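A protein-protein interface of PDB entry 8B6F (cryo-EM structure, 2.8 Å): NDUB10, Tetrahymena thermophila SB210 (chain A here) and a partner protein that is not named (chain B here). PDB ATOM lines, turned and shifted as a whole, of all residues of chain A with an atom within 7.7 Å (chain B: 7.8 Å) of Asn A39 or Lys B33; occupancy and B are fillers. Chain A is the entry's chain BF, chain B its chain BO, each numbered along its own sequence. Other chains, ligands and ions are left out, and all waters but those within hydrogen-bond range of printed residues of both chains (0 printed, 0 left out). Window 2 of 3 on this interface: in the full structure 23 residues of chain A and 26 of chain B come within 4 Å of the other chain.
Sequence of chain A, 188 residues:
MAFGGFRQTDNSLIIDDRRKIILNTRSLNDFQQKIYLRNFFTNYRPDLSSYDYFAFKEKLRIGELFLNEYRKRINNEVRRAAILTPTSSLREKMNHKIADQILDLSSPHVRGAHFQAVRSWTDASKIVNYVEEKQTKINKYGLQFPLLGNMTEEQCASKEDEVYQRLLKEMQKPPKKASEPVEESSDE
Along chain A the printed residues that touch a printed residue of chain B span positions 39 to 47.
Of the 15 printed residues of chain B, 6 touch a printed residue of chain A.
Hydrophobic or aromatic side chains of chain B that line the printed part of chain A: Val B28 and Ala B29.
Among the printed residues, 8 pairs touch across the chains.
Among the printed residues, no Asp or Glu carboxylate lies within 4 Å of a Lys or Arg side-chain nitrogen of the other chain.
Asn A39 touches just one residue of chain B: Lys B33 (3.5 Å).
Lys B33 touches one residue of chain A.
Of the printed residues of chain A, Ala B29 touches Phe A41, Pro A46 and Asp A47.
Of the printed residues of chain B, Phe A41 touches Ala B29 and Asn B30.
Of the printed residues of chain B, Asp A47 touches Val B28, Ala B29, Asn B32 and Arg B117.
The nearest printed residue of chain A that does not touch Ala B29 is Asn A39 (7.6 Å).
O of Asp A47 is in hydrogen-bond range of ND2 of Asn B32 (3.1 Å).
O of Asp A47 lies within hydrogen-bond range of NH2 of Arg B117 (3.1 Å).
O of Asn A39 touches NZ of Lys B33, 3.5 Å away.
Phe A41 touches Ala B29.
OD1 of Asn B30 touches CZ of Phe A41, 3.1 Å away.
Pro A46 touches Ala B29.
CG1 of Val B28 touches CB of Asp A47, 3.6 Å away.
Asp A47 touches Ala B29 (N to CB, 3.8 Å).
O of Ile A35 sits at hydrogen-bond distance from ND2 of Asn A39, 2.9 Å away.
The backbone carbonyl oxygen (O) of Tyr A36 is in hydrogen-bond range of the side-chain amide nitrogen (ND2) of Asn A39, at 2.7 Å.
The side-chain amide oxygen of Asn B30 sits close to the backbone carbonyl oxygen of Arg B26 (3.0 Å).
ND2 of Asn B32 sits at hydrogen-bond distance from O of Val B28, 3.1 Å away.
ND2 of Asn B32 lies close to NH2 of Arg B117 (3.0 Å).
The side-chain sulfur (SG) of Cys B78 forms a disulfide with the side-chain sulfur (SG) of Cys B35 (2.0 Å).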
ATOM      1  N   ASP A  16      -8.876  -0.130  34.927  1.00  0.00           N
ATOM      2  CA  ASP A  16      -9.665  -0.427  33.737  1.00  0.00           C
ATOM      3  C   ASP A  16     -10.015   0.893  33.064  1.00  0.00           C
ATOM      4  O   ASP A  16     -10.877   1.634  33.544  1.00  0.00           O
ATOM      5  CB  ASP A  16     -10.924  -1.215  34.092  1.00  0.00           C
ATOM      6  CG  ASP A  16     -11.685  -1.674  32.862  1.00  0.00           C
ATOM      7  OD1 ASP A  16     -11.263  -2.664  32.230  1.00  0.00           O
ATOM      8  OD2 ASP A  16     -12.703  -1.040  32.520  1.00  0.00           O
ATOM      9  N   GLN A  32     -15.810  -9.751  38.747  1.00  0.00           N
ATOM     10  CA  GLN A  32     -14.669  -8.896  38.443  1.00  0.00           C
ATOM     11  C   GLN A  32     -13.439  -9.727  38.109  1.00  0.00           C
ATOM     12  O   GLN A  32     -12.669  -9.375  37.209  1.00  0.00           O
ATOM     13  CB  GLN A  32     -14.392  -7.955  39.613  1.00  0.00           C
ATOM     14  CG  GLN A  32     -15.496  -6.936  39.837  1.00  0.00           C
ATOM     15  CD  GLN A  32     -15.261  -6.081  41.061  1.00  0.00           C
ATOM     16  OE1 GLN A  32     -14.319  -6.306  41.816  1.00  0.00           O
ATOM     17  NE2 GLN A  32     -16.119  -5.091  41.263  1.00  0.00           N
ATOM     18  N   GLN A  33     -13.234 -10.833  38.823  1.00  0.00           N
ATOM     19  CA  GLN A  33     -12.143 -11.736  38.478  1.00  0.00           C
ATOM     20  C   GLN A  33     -12.315 -12.275  37.065  1.00  0.00           C
ATOM     21  O   GLN A  33     -11.362 -12.308  36.280  1.00  0.00           O
ATOM     22  CB  GLN A  33     -12.072 -12.885  39.484  1.00  0.00           C
ATOM     23  CG  GLN A  33     -11.548 -12.487  40.846  1.00  0.00           C
ATOM     24  CD  GLN A  33     -11.706 -13.593  41.865  1.00  0.00           C
ATOM     25  OE1 GLN A  33     -11.795 -14.766  41.513  1.00  0.00           O
ATOM     26  NE2 GLN A  33     -11.745 -13.222  43.137  1.00  0.00           N
ATOM     27  N   LYS A  34     -13.533 -12.694  36.720  1.00  0.00           N
ATOM     28  CA  LYS A  34     -13.793 -13.187  35.371  1.00  0.00           C
ATOM     29  C   LYS A  34     -13.472 -12.123  34.328  1.00  0.00           C
ATOM     30  O   LYS A  34     -12.874 -12.424  33.289  1.00  0.00           O
ATOM     31  CB  LYS A  34     -15.255 -13.628  35.261  1.00  0.00           C
ATOM     32  CG  LYS A  34     -15.763 -13.874  33.843  1.00  0.00           C
ATOM     33  CD  LYS A  34     -15.047 -15.028  33.161  1.00  0.00           C
ATOM     34  CE  LYS A  34     -15.484 -16.366  33.733  1.00  0.00           C
ATOM     35  NZ  LYS A  34     -14.903 -17.505  32.971  1.00  0.00           N
ATOM     36  N   ILE A  35     -13.862 -10.875  34.588  1.00  0.00           N
ATOM     37  CA  ILE A  35     -13.707  -9.820  33.590  1.00  0.00           C
ATOM     38  C   ILE A  35     -12.237  -9.463  33.404  1.00  0.00           C
ATOM     39  O   ILE A  35     -11.759  -9.313  32.275  1.00  0.00           O
ATOM     40  CB  ILE A  35     -14.539  -8.587  33.991  1.00  0.00           C
ATOM     41  CG1 ILE A  35     -16.038  -8.885  33.899  1.00  0.00           C
ATOM     42  CG2 ILE A  35     -14.184  -7.379  33.130  1.00  0.00           C
ATOM     43  CD1 ILE A  35     -16.531  -9.221  32.508  1.00  0.00           C
ATOM     44  N   TYR A  36     -11.501  -9.312  34.504  1.00  0.00           N
ATOM     45  CA  TYR A  36     -10.133  -8.808  34.432  1.00  0.00           C
ATOM     46  C   TYR A  36      -9.124  -9.949  34.338  1.00  0.00           C
ATOM     47  O   TYR A  36      -8.360 -10.031  33.372  1.00  0.00           O
ATOM     48  CB  TYR A  36      -9.856  -7.914  35.644  1.00  0.00           C
ATOM     49  CG  TYR A  36     -10.807  -6.742  35.710  1.00  0.00           C
ATOM     50  CD1 TYR A  36     -11.051  -5.959  34.588  1.00  0.00           C
ATOM     51  CD2 TYR A  36     -11.488  -6.440  36.879  1.00  0.00           C
ATOM     52  CE1 TYR A  36     -11.928  -4.900  34.633  1.00  0.00           C
ATOM     53  CE2 TYR A  36     -12.368  -5.381  36.934  1.00  0.00           C
ATOM     54  CZ  TYR A  36     -12.583  -4.616  35.807  1.00  0.00           C
ATOM     55  OH  TYR A  36     -13.460  -3.563  35.860  1.00  0.00           O
ATOM     56  N   LEU A  37      -9.109 -10.831  35.329  1.00  0.00           N
ATOM     57  CA  LEU A  37      -8.364 -12.069  35.195  1.00  0.00           C
ATOM     58  C   LEU A  37      -9.186 -13.070  34.385  1.00  0.00           C
ATOM     59  O   LEU A  37     -10.358 -12.846  34.077  1.00  0.00           O
ATOM     60  CB  LEU A  37      -8.022 -12.642  36.568  1.00  0.00           C
ATOM     61  CG  LEU A  37      -7.512 -11.642  37.608  1.00  0.00           C
ATOM     62  CD1 LEU A  37      -7.322 -12.323  38.952  1.00  0.00           C
ATOM     63  CD2 LEU A  37      -6.220 -10.988  37.150  1.00  0.00           C
ATOM     64  N   ARG A  38      -8.556 -14.182  34.021  1.00  0.00           N
ATOM     65  CA  ARG A  38      -9.198 -15.292  33.326  1.00  0.00           C
ATOM     66  C   ARG A  38      -9.677 -14.930  31.927  1.00  0.00           C
ATOM     67  O   ARG A  38     -10.257 -15.786  31.253  1.00  0.00           O
ATOM     68  CB  ARG A  38     -10.398 -15.843  34.109  1.00  0.00           C
ATOM     69  CG  ARG A  38     -10.084 -16.234  35.542  1.00  0.00           C
ATOM     70  CD  ARG A  38     -11.283 -16.892  36.202  1.00  0.00           C
ATOM     71  NE  ARG A  38     -10.893 -17.726  37.333  1.00  0.00           N
ATOM     72  CZ  ARG A  38     -10.830 -17.317  38.593  1.00  0.00           C
ATOM     73  NH1 ARG A  38     -11.131 -16.077  38.935  1.00  0.00           N
ATOM     74  NH2 ARG A  38     -10.455 -18.178  39.533  1.00  0.00           N
ATOM     75  N   ASN A  39      -9.456 -13.704  31.463  1.00  0.00           N
ATOM     76  CA  ASN A  39      -9.939 -13.271  30.158  1.00  0.00           C
ATOM     77  C   ASN A  39      -8.975 -13.601  29.028  1.00  0.00           C
ATOM     78  O   ASN A  39      -9.261 -13.271  27.873  1.00  0.00           O
ATOM     79  CB  ASN A  39     -10.220 -11.765  30.170  1.00  0.00           C
ATOM     80  CG  ASN A  39      -9.010 -10.946  30.574  1.00  0.00           C
ATOM     81  OD1 ASN A  39      -7.897 -11.462  30.664  1.00  0.00           O
ATOM     82  ND2 ASN A  39      -9.222  -9.660  30.816  1.00  0.00           N
ATOM     83  N   PHE A  40      -7.846 -14.235  29.327  1.00  0.00           N
ATOM     84  CA  PHE A  40      -6.900 -14.605  28.289  1.00  0.00           C
ATOM     85  C   PHE A  40      -7.460 -15.737  27.432  1.00  0.00           C
ATOM     86  O   PHE A  40      -8.426 -16.412  27.796  1.00  0.00           O
ATOM     87  CB  PHE A  40      -5.565 -15.021  28.905  1.00  0.00           C
ATOM     88  CG  PHE A  40      -5.677 -16.144  29.896  1.00  0.00           C
ATOM     89  CD1 PHE A  40      -5.604 -17.462  29.481  1.00  0.00           C
ATOM     90  CD2 PHE A  40      -5.839 -15.879  31.246  1.00  0.00           C
ATOM     91  CE1 PHE A  40      -5.705 -18.494  30.390  1.00  0.00           C
ATOM     92  CE2 PHE A  40      -5.939 -16.906  32.159  1.00  0.00           C
ATOM     93  CZ  PHE A  40      -5.870 -18.215  31.731  1.00  0.00           C
ATOM     94  N   PHE A  41      -6.839 -15.936  26.275  1.00  0.00           N
ATOM     95  CA  PHE A  41      -7.258 -16.947  25.318  1.00  0.00           C
ATOM     96  C   PHE A  41      -6.439 -18.220  25.499  1.00  0.00           C
ATOM     97  O   PHE A  41      -5.264 -18.176  25.870  1.00  0.00           O
ATOM     98  CB  PHE A  41      -7.105 -16.431  23.886  1.00  0.00           C
ATOM     99  CG  PHE A  41      -7.925 -15.206  23.590  1.00  0.00           C
ATOM    100  CD1 PHE A  41      -9.163 -15.018  24.181  1.00  0.00           C
ATOM    101  CD2 PHE A  41      -7.454 -14.241  22.714  1.00  0.00           C
ATOM    102  CE1 PHE A  41      -9.916 -13.893  23.905  1.00  0.00           C
ATOM    103  CE2 PHE A  41      -8.202 -13.115  22.432  1.00  0.00           C
ATOM    104  CZ  PHE A  41      -9.434 -12.941  23.029  1.00  0.00           C
ATOM    105  N   THR A  42      -7.077 -19.361  25.232  1.00  0.00           N
ATOM    106  CA  THR A  42      -6.454 -20.667  25.416  1.00  0.00           C
ATOM    107  C   THR A  42      -6.635 -21.555  24.189  1.00  0.00           C
ATOM    108  O   THR A  42      -6.643 -22.782  24.304  1.00  0.00           O
ATOM    109  CB  THR A  42      -7.012 -21.365  26.657  1.00  0.00           C
ATOM    110  OG1 THR A  42      -8.436 -21.483  26.546  1.00  0.00           O
ATOM    111  CG2 THR A  42      -6.665 -20.582  27.912  1.00  0.00           C
ATOM    112  N   PRO A  46      -9.922 -18.245  19.241  1.00  0.00           N
ATOM    113  CA  PRO A  46     -11.021 -18.017  20.193  1.00  0.00           C
ATOM    114  C   PRO A  46     -12.225 -17.335  19.574  1.00  0.00           C
ATOM    115  O   PRO A  46     -13.324 -17.426  20.134  1.00  0.00           O
ATOM    116  CB  PRO A  46     -10.372 -17.139  21.272  1.00  0.00           C
ATOM    117  CG  PRO A  46      -9.252 -16.460  20.573  1.00  0.00           C
ATOM    118  CD  PRO A  46      -8.739 -17.430  19.558  1.00  0.00           C
ATOM    119  N   ASP A  47     -12.055 -16.647  18.446  1.00  0.00           N
ATOM    120  CA  ASP A  47     -13.182 -15.956  17.828  1.00  0.00           C
ATOM    121  C   ASP A  47     -14.252 -16.932  17.357  1.00  0.00           C
ATOM    122  O   ASP A  47     -15.436 -16.581  17.320  1.00  0.00           O
ATOM    123  CB  ASP A  47     -12.693 -15.097  16.663  1.00  0.00           C
ATOM    124  CG  ASP A  47     -11.862 -15.881  15.671  1.00  0.00           C
ATOM    125  OD1 ASP A  47     -11.235 -16.878  16.081  1.00  0.00           O
ATOM    126  OD2 ASP A  47     -11.831 -15.501  14.484  1.00  0.00           O
ATOM    127  N   ARG B  26      -8.995 -10.815  18.194  1.00  0.00           N
ATOM    128  CA  ARG B  26      -9.232 -10.429  19.580  1.00  0.00           C
ATOM    129  C   ARG B  26     -10.567  -9.713  19.729  1.00  0.00           C
ATOM    130  O   ARG B  26     -11.331  -9.998  20.659  1.00  0.00           O
ATOM    131  CB  ARG B  26      -8.090  -9.542  20.079  1.00  0.00           C
ATOM    132  CG  ARG B  26      -8.386  -8.853  21.401  1.00  0.00           C
ATOM    133  CD  ARG B  26      -7.153  -8.183  21.976  1.00  0.00           C
ATOM    134  NE  ARG B  26      -6.605  -7.170  21.081  1.00  0.00           N
ATOM    135  CZ  ARG B  26      -5.611  -7.372  20.227  1.00  0.00           C
ATOM    136  NH1 ARG B  26      -5.024  -8.552  20.110  1.00  0.00           N
ATOM    137  NH2 ARG B  26      -5.192  -6.363  19.469  1.00  0.00           N
ATOM    138  N   PHE B  27     -10.867  -8.782  18.824  1.00  0.00           N
ATOM    139  CA  PHE B  27     -12.128  -8.052  18.907  1.00  0.00           C
ATOM    140  C   PHE B  27     -13.316  -8.998  18.802  1.00  0.00           C
ATOM    141  O   PHE B  27     -14.263  -8.915  19.592  1.00  0.00           O
ATOM    142  CB  PHE B  27     -12.183  -6.990  17.810  1.00  0.00           C
ATOM    143  CG  PHE B  27     -13.500  -6.282  17.721  1.00  0.00           C
ATOM    144  CD1 PHE B  27     -13.776  -5.204  18.542  1.00  0.00           C
ATOM    145  CD2 PHE B  27     -14.460  -6.687  16.808  1.00  0.00           C
ATOM    146  CE1 PHE B  27     -14.986  -4.546  18.462  1.00  0.00           C
ATOM    147  CE2 PHE B  27     -15.673  -6.034  16.723  1.00  0.00           C
ATOM    148  CZ  PHE B  27     -15.936  -4.962  17.551  1.00  0.00           C
ATOM    149  N   VAL B  28     -13.285  -9.912  17.830  1.00  0.00           N
ATOM    150  CA  VAL B  28     -14.409 -10.825  17.637  1.00  0.00           C
ATOM    151  C   VAL B  28     -14.570 -11.732  18.850  1.00  0.00           C
ATOM    152  O   VAL B  28     -15.687 -11.968  19.323  1.00  0.00           O
ATOM    153  CB  VAL B  28     -14.224 -11.634  16.340  1.00  0.00           C
ATOM    154  CG1 VAL B  28     -15.301 -12.703  16.208  1.00  0.00           C
ATOM    155  CG2 VAL B  28     -14.260 -10.713  15.135  1.00  0.00           C
ATOM    156  N   ALA B  29     -13.461 -12.258  19.371  1.00  0.00           N
ATOM    157  CA  ALA B  29     -13.543 -13.151  20.522  1.00  0.00           C
ATOM    158  C   ALA B  29     -14.111 -12.426  21.736  1.00  0.00           C
ATOM    159  O   ALA B  29     -14.989 -12.949  22.430  1.00  0.00           O
ATOM    160  CB  ALA B  29     -12.162 -13.727  20.835  1.00  0.00           C
ATOM    161  N   ASN B  30     -13.609 -11.223  22.019  1.00  0.00           N
ATOM    162  CA  ASN B  30     -14.102 -10.479  23.173  1.00  0.00           C
ATOM    163  C   ASN B  30     -15.580 -10.148  23.027  1.00  0.00           C
ATOM    164  O   ASN B  30     -16.355 -10.309  23.974  1.00  0.00           O
ATOM    165  CB  ASN B  30     -13.291  -9.197  23.356  1.00  0.00           C
ATOM    166  CG  ASN B  30     -11.847  -9.467  23.704  1.00  0.00           C
ATOM    167  OD1 ASN B  30     -11.377 -10.599  23.614  1.00  0.00           O
ATOM    168  ND2 ASN B  30     -11.131  -8.426  24.106  1.00  0.00           N
ATOM    169  N   LYS B  31     -15.989  -9.686  21.845  1.00  0.00           N
ATOM    170  CA  LYS B  31     -17.385  -9.308  21.648  1.00  0.00           C
ATOM    171  C   LYS B  31     -18.305 -10.521  21.709  1.00  0.00           C
ATOM    172  O   LYS B  31     -19.415 -10.433  22.242  1.00  0.00           O
ATOM    173  CB  LYS B  31     -17.548  -8.570  20.320  1.00  0.00           C
ATOM    174  CG  LYS B  31     -16.891  -7.195  20.293  1.00  0.00           C
ATOM    175  CD  LYS B  31     -17.488  -6.264  21.340  1.00  0.00           C
ATOM    176  CE  LYS B  31     -16.893  -4.871  21.247  1.00  0.00           C
ATOM    177  NZ  LYS B  31     -17.424  -3.975  22.311  1.00  0.00           N
ATOM    178  N   ASN B  32     -17.867 -11.661  21.172  1.00  0.00           N
ATOM    179  CA  ASN B  32     -18.675 -12.870  21.290  1.00  0.00           C
ATOM    180  C   ASN B  32     -18.831 -13.284  22.746  1.00  0.00           C
ATOM    181  O   ASN B  32     -19.924 -13.664  23.177  1.00  0.00           O
ATOM    182  CB  ASN B  32     -18.053 -14.005  20.475  1.00  0.00           C
ATOM    183  CG  ASN B  32     -18.310 -13.864  18.988  1.00  0.00           C
ATOM    184  OD1 ASN B  32     -19.357 -13.374  18.572  1.00  0.00           O
ATOM    185  ND2 ASN B  32     -17.355 -14.307  18.180  1.00  0.00           N
ATOM    186  N   LYS B  33     -17.745 -13.226  23.517  1.00  0.00           N
ATOM    187  CA  LYS B  33     -17.833 -13.593  24.926  1.00  0.00           C
ATOM    188  C   LYS B  33     -18.766 -12.655  25.681  1.00  0.00           C
ATOM    189  O   LYS B  33     -19.498 -13.085  26.579  1.00  0.00           O
ATOM    190  CB  LYS B  33     -16.438 -13.587  25.549  1.00  0.00           C
ATOM    191  CG  LYS B  33     -16.418 -13.883  27.037  1.00  0.00           C
ATOM    192  CD  LYS B  33     -15.092 -14.501  27.463  1.00  0.00           C
ATOM    193  CE  LYS B  33     -13.906 -13.602  27.135  1.00  0.00           C
ATOM    194  NZ  LYS B  33     -12.616 -14.230  27.538  1.00  0.00           N
ATOM    195  N   GLU B  34     -18.748 -11.366  25.335  1.00  0.00           N
ATOM    196  CA  GLU B  34     -19.588 -10.398  26.030  1.00  0.00           C
ATOM    197  C   GLU B  34     -21.047 -10.474  25.598  1.00  0.00           C
ATOM    198  O   GLU B  34     -21.940 -10.253  26.423  1.00  0.00           O
ATOM    199  CB  GLU B  34     -19.056  -8.984  25.800  1.00  0.00           C
ATOM    200  CG  GLU B  34     -17.701  -8.724  26.434  1.00  0.00           C
ATOM    201  CD  GLU B  34     -17.189  -7.327  26.156  1.00  0.00           C
ATOM    202  OE1 GLU B  34     -17.947  -6.522  25.579  1.00  0.00           O
ATOM    203  OE2 GLU B  34     -16.028  -7.035  26.512  1.00  0.00           O
ATOM    204  N   CYS B  35     -21.312 -10.777  24.328  1.00  0.00           N
ATOM    205  CA  CYS B  35     -22.657 -10.685  23.774  1.00  0.00           C
ATOM    206  C   CYS B  35     -23.280 -12.046  23.489  1.00  0.00           C
ATOM    207  O   CYS B  35     -24.325 -12.108  22.832  1.00  0.00           O
ATOM    208  CB  CYS B  35     -22.637  -9.855  22.488  1.00  0.00           C
ATOM    209  SG  CYS B  35     -21.559  -8.406  22.530  1.00  0.00           S
ATOM    210  N   GLY B  36     -22.675 -13.134  23.960  1.00  0.00           N
ATOM    211  CA  GLY B  36     -23.236 -14.449  23.702  1.00  0.00           C
ATOM    212  C   GLY B  36     -24.644 -14.627  24.225  1.00  0.00           C
ATOM    213  O   GLY B  36     -25.379 -15.484  23.725  1.00  0.00           O
ATOM    214  N   TYR B  37     -25.039 -13.836  25.222  1.00  0.00           N
ATOM    215  CA  TYR B  37     -26.401 -13.916  25.738  1.00  0.00           C
ATOM    216  C   TYR B  37     -27.418 -13.588  24.655  1.00  0.00           C
ATOM    217  O   TYR B  37     -28.468 -14.232  24.559  1.00  0.00           O
ATOM    218  CB  TYR B  37     -26.549 -12.969  26.928  1.00  0.00           C
ATOM    219  CG  TYR B  37     -27.943 -12.884  27.496  1.00  0.00           C
ATOM    220  CD1 TYR B  37     -28.405 -13.838  28.391  1.00  0.00           C
ATOM    221  CD2 TYR B  37     -28.787 -11.837  27.158  1.00  0.00           C
ATOM    222  CE1 TYR B  37     -29.674 -13.760  28.921  1.00  0.00           C
ATOM    223  CE2 TYR B  37     -30.058 -11.750  27.684  1.00  0.00           C
ATOM    224  CZ  TYR B  37     -30.494 -12.714  28.567  1.00  0.00           C
ATOM    225  OH  TYR B  37     -31.757 -12.634  29.094  1.00  0.00           O
ATOM    226  N   CYS B  78     -24.183  -4.565  20.507  1.00  0.00           N
ATOM    227  CA  CYS B  78     -23.162  -5.114  21.393  1.00  0.00           C
ATOM    228  C   CYS B  78     -21.912  -5.507  20.618  1.00  0.00           C
ATOM    229  O   CYS B  78     -20.788  -5.246  21.061  1.00  0.00           O
ATOM    230  CB  CYS B  78     -23.729  -6.316  22.149  1.00  0.00           C
ATOM    231  SG  CYS B  78     -22.663  -6.973  23.451  1.00  0.00           S
ATOM    232  N   MET B  79     -22.085  -6.130  19.450  1.00  0.00           N
ATOM    233  CA  MET B  79     -20.932  -6.557  18.665  1.00  0.00           C
ATOM    234  C   MET B  79     -20.171  -5.366  18.097  1.00  0.00           C
ATOM    235  O   MET B  79     -18.938  -5.394  18.018  1.00  0.00           O
ATOM    236  CB  MET B  79     -21.383  -7.484  17.535  1.00  0.00           C
ATOM    237  CG  MET B  79     -21.931  -8.823  18.004  1.00  0.00           C
ATOM    238  SD  MET B  79     -20.728  -9.814  18.908  1.00  0.00           S
ATOM    239  CE  MET B  79     -19.473 -10.074  17.657  1.00  0.00           C
ATOM    240  N   ARG B 117     -24.462 -17.850  12.960  1.00  0.00           N
ATOM    241  CA  ARG B 117     -23.435 -17.072  13.645  1.00  0.00           C
ATOM    242  C   ARG B 117     -22.252 -16.797  12.732  1.00  0.00           C
ATOM    243  O   ARG B 117     -21.580 -15.769  12.877  1.00  0.00           O
ATOM    244  CB  ARG B 117     -22.959 -17.795  14.905  1.00  0.00           C
ATOM    245  CG  ARG B 117     -21.592 -17.317  15.385  1.00  0.00           C
ATOM    246  CD  ARG B 117     -21.279 -17.781  16.792  1.00  0.00           C
ATOM    247  NE  ARG B 117     -19.938 -17.377  17.200  1.00  0.00           N
ATOM    248  CZ  ARG B 117     -19.459 -17.492  18.432  1.00  0.00           C
ATOM    249  NH1 ARG B 117     -20.193 -17.982  19.416  1.00  0.00           N
ATOM    250  NH2 ARG B 117     -18.209 -17.110  18.680  1.00  0.00           N
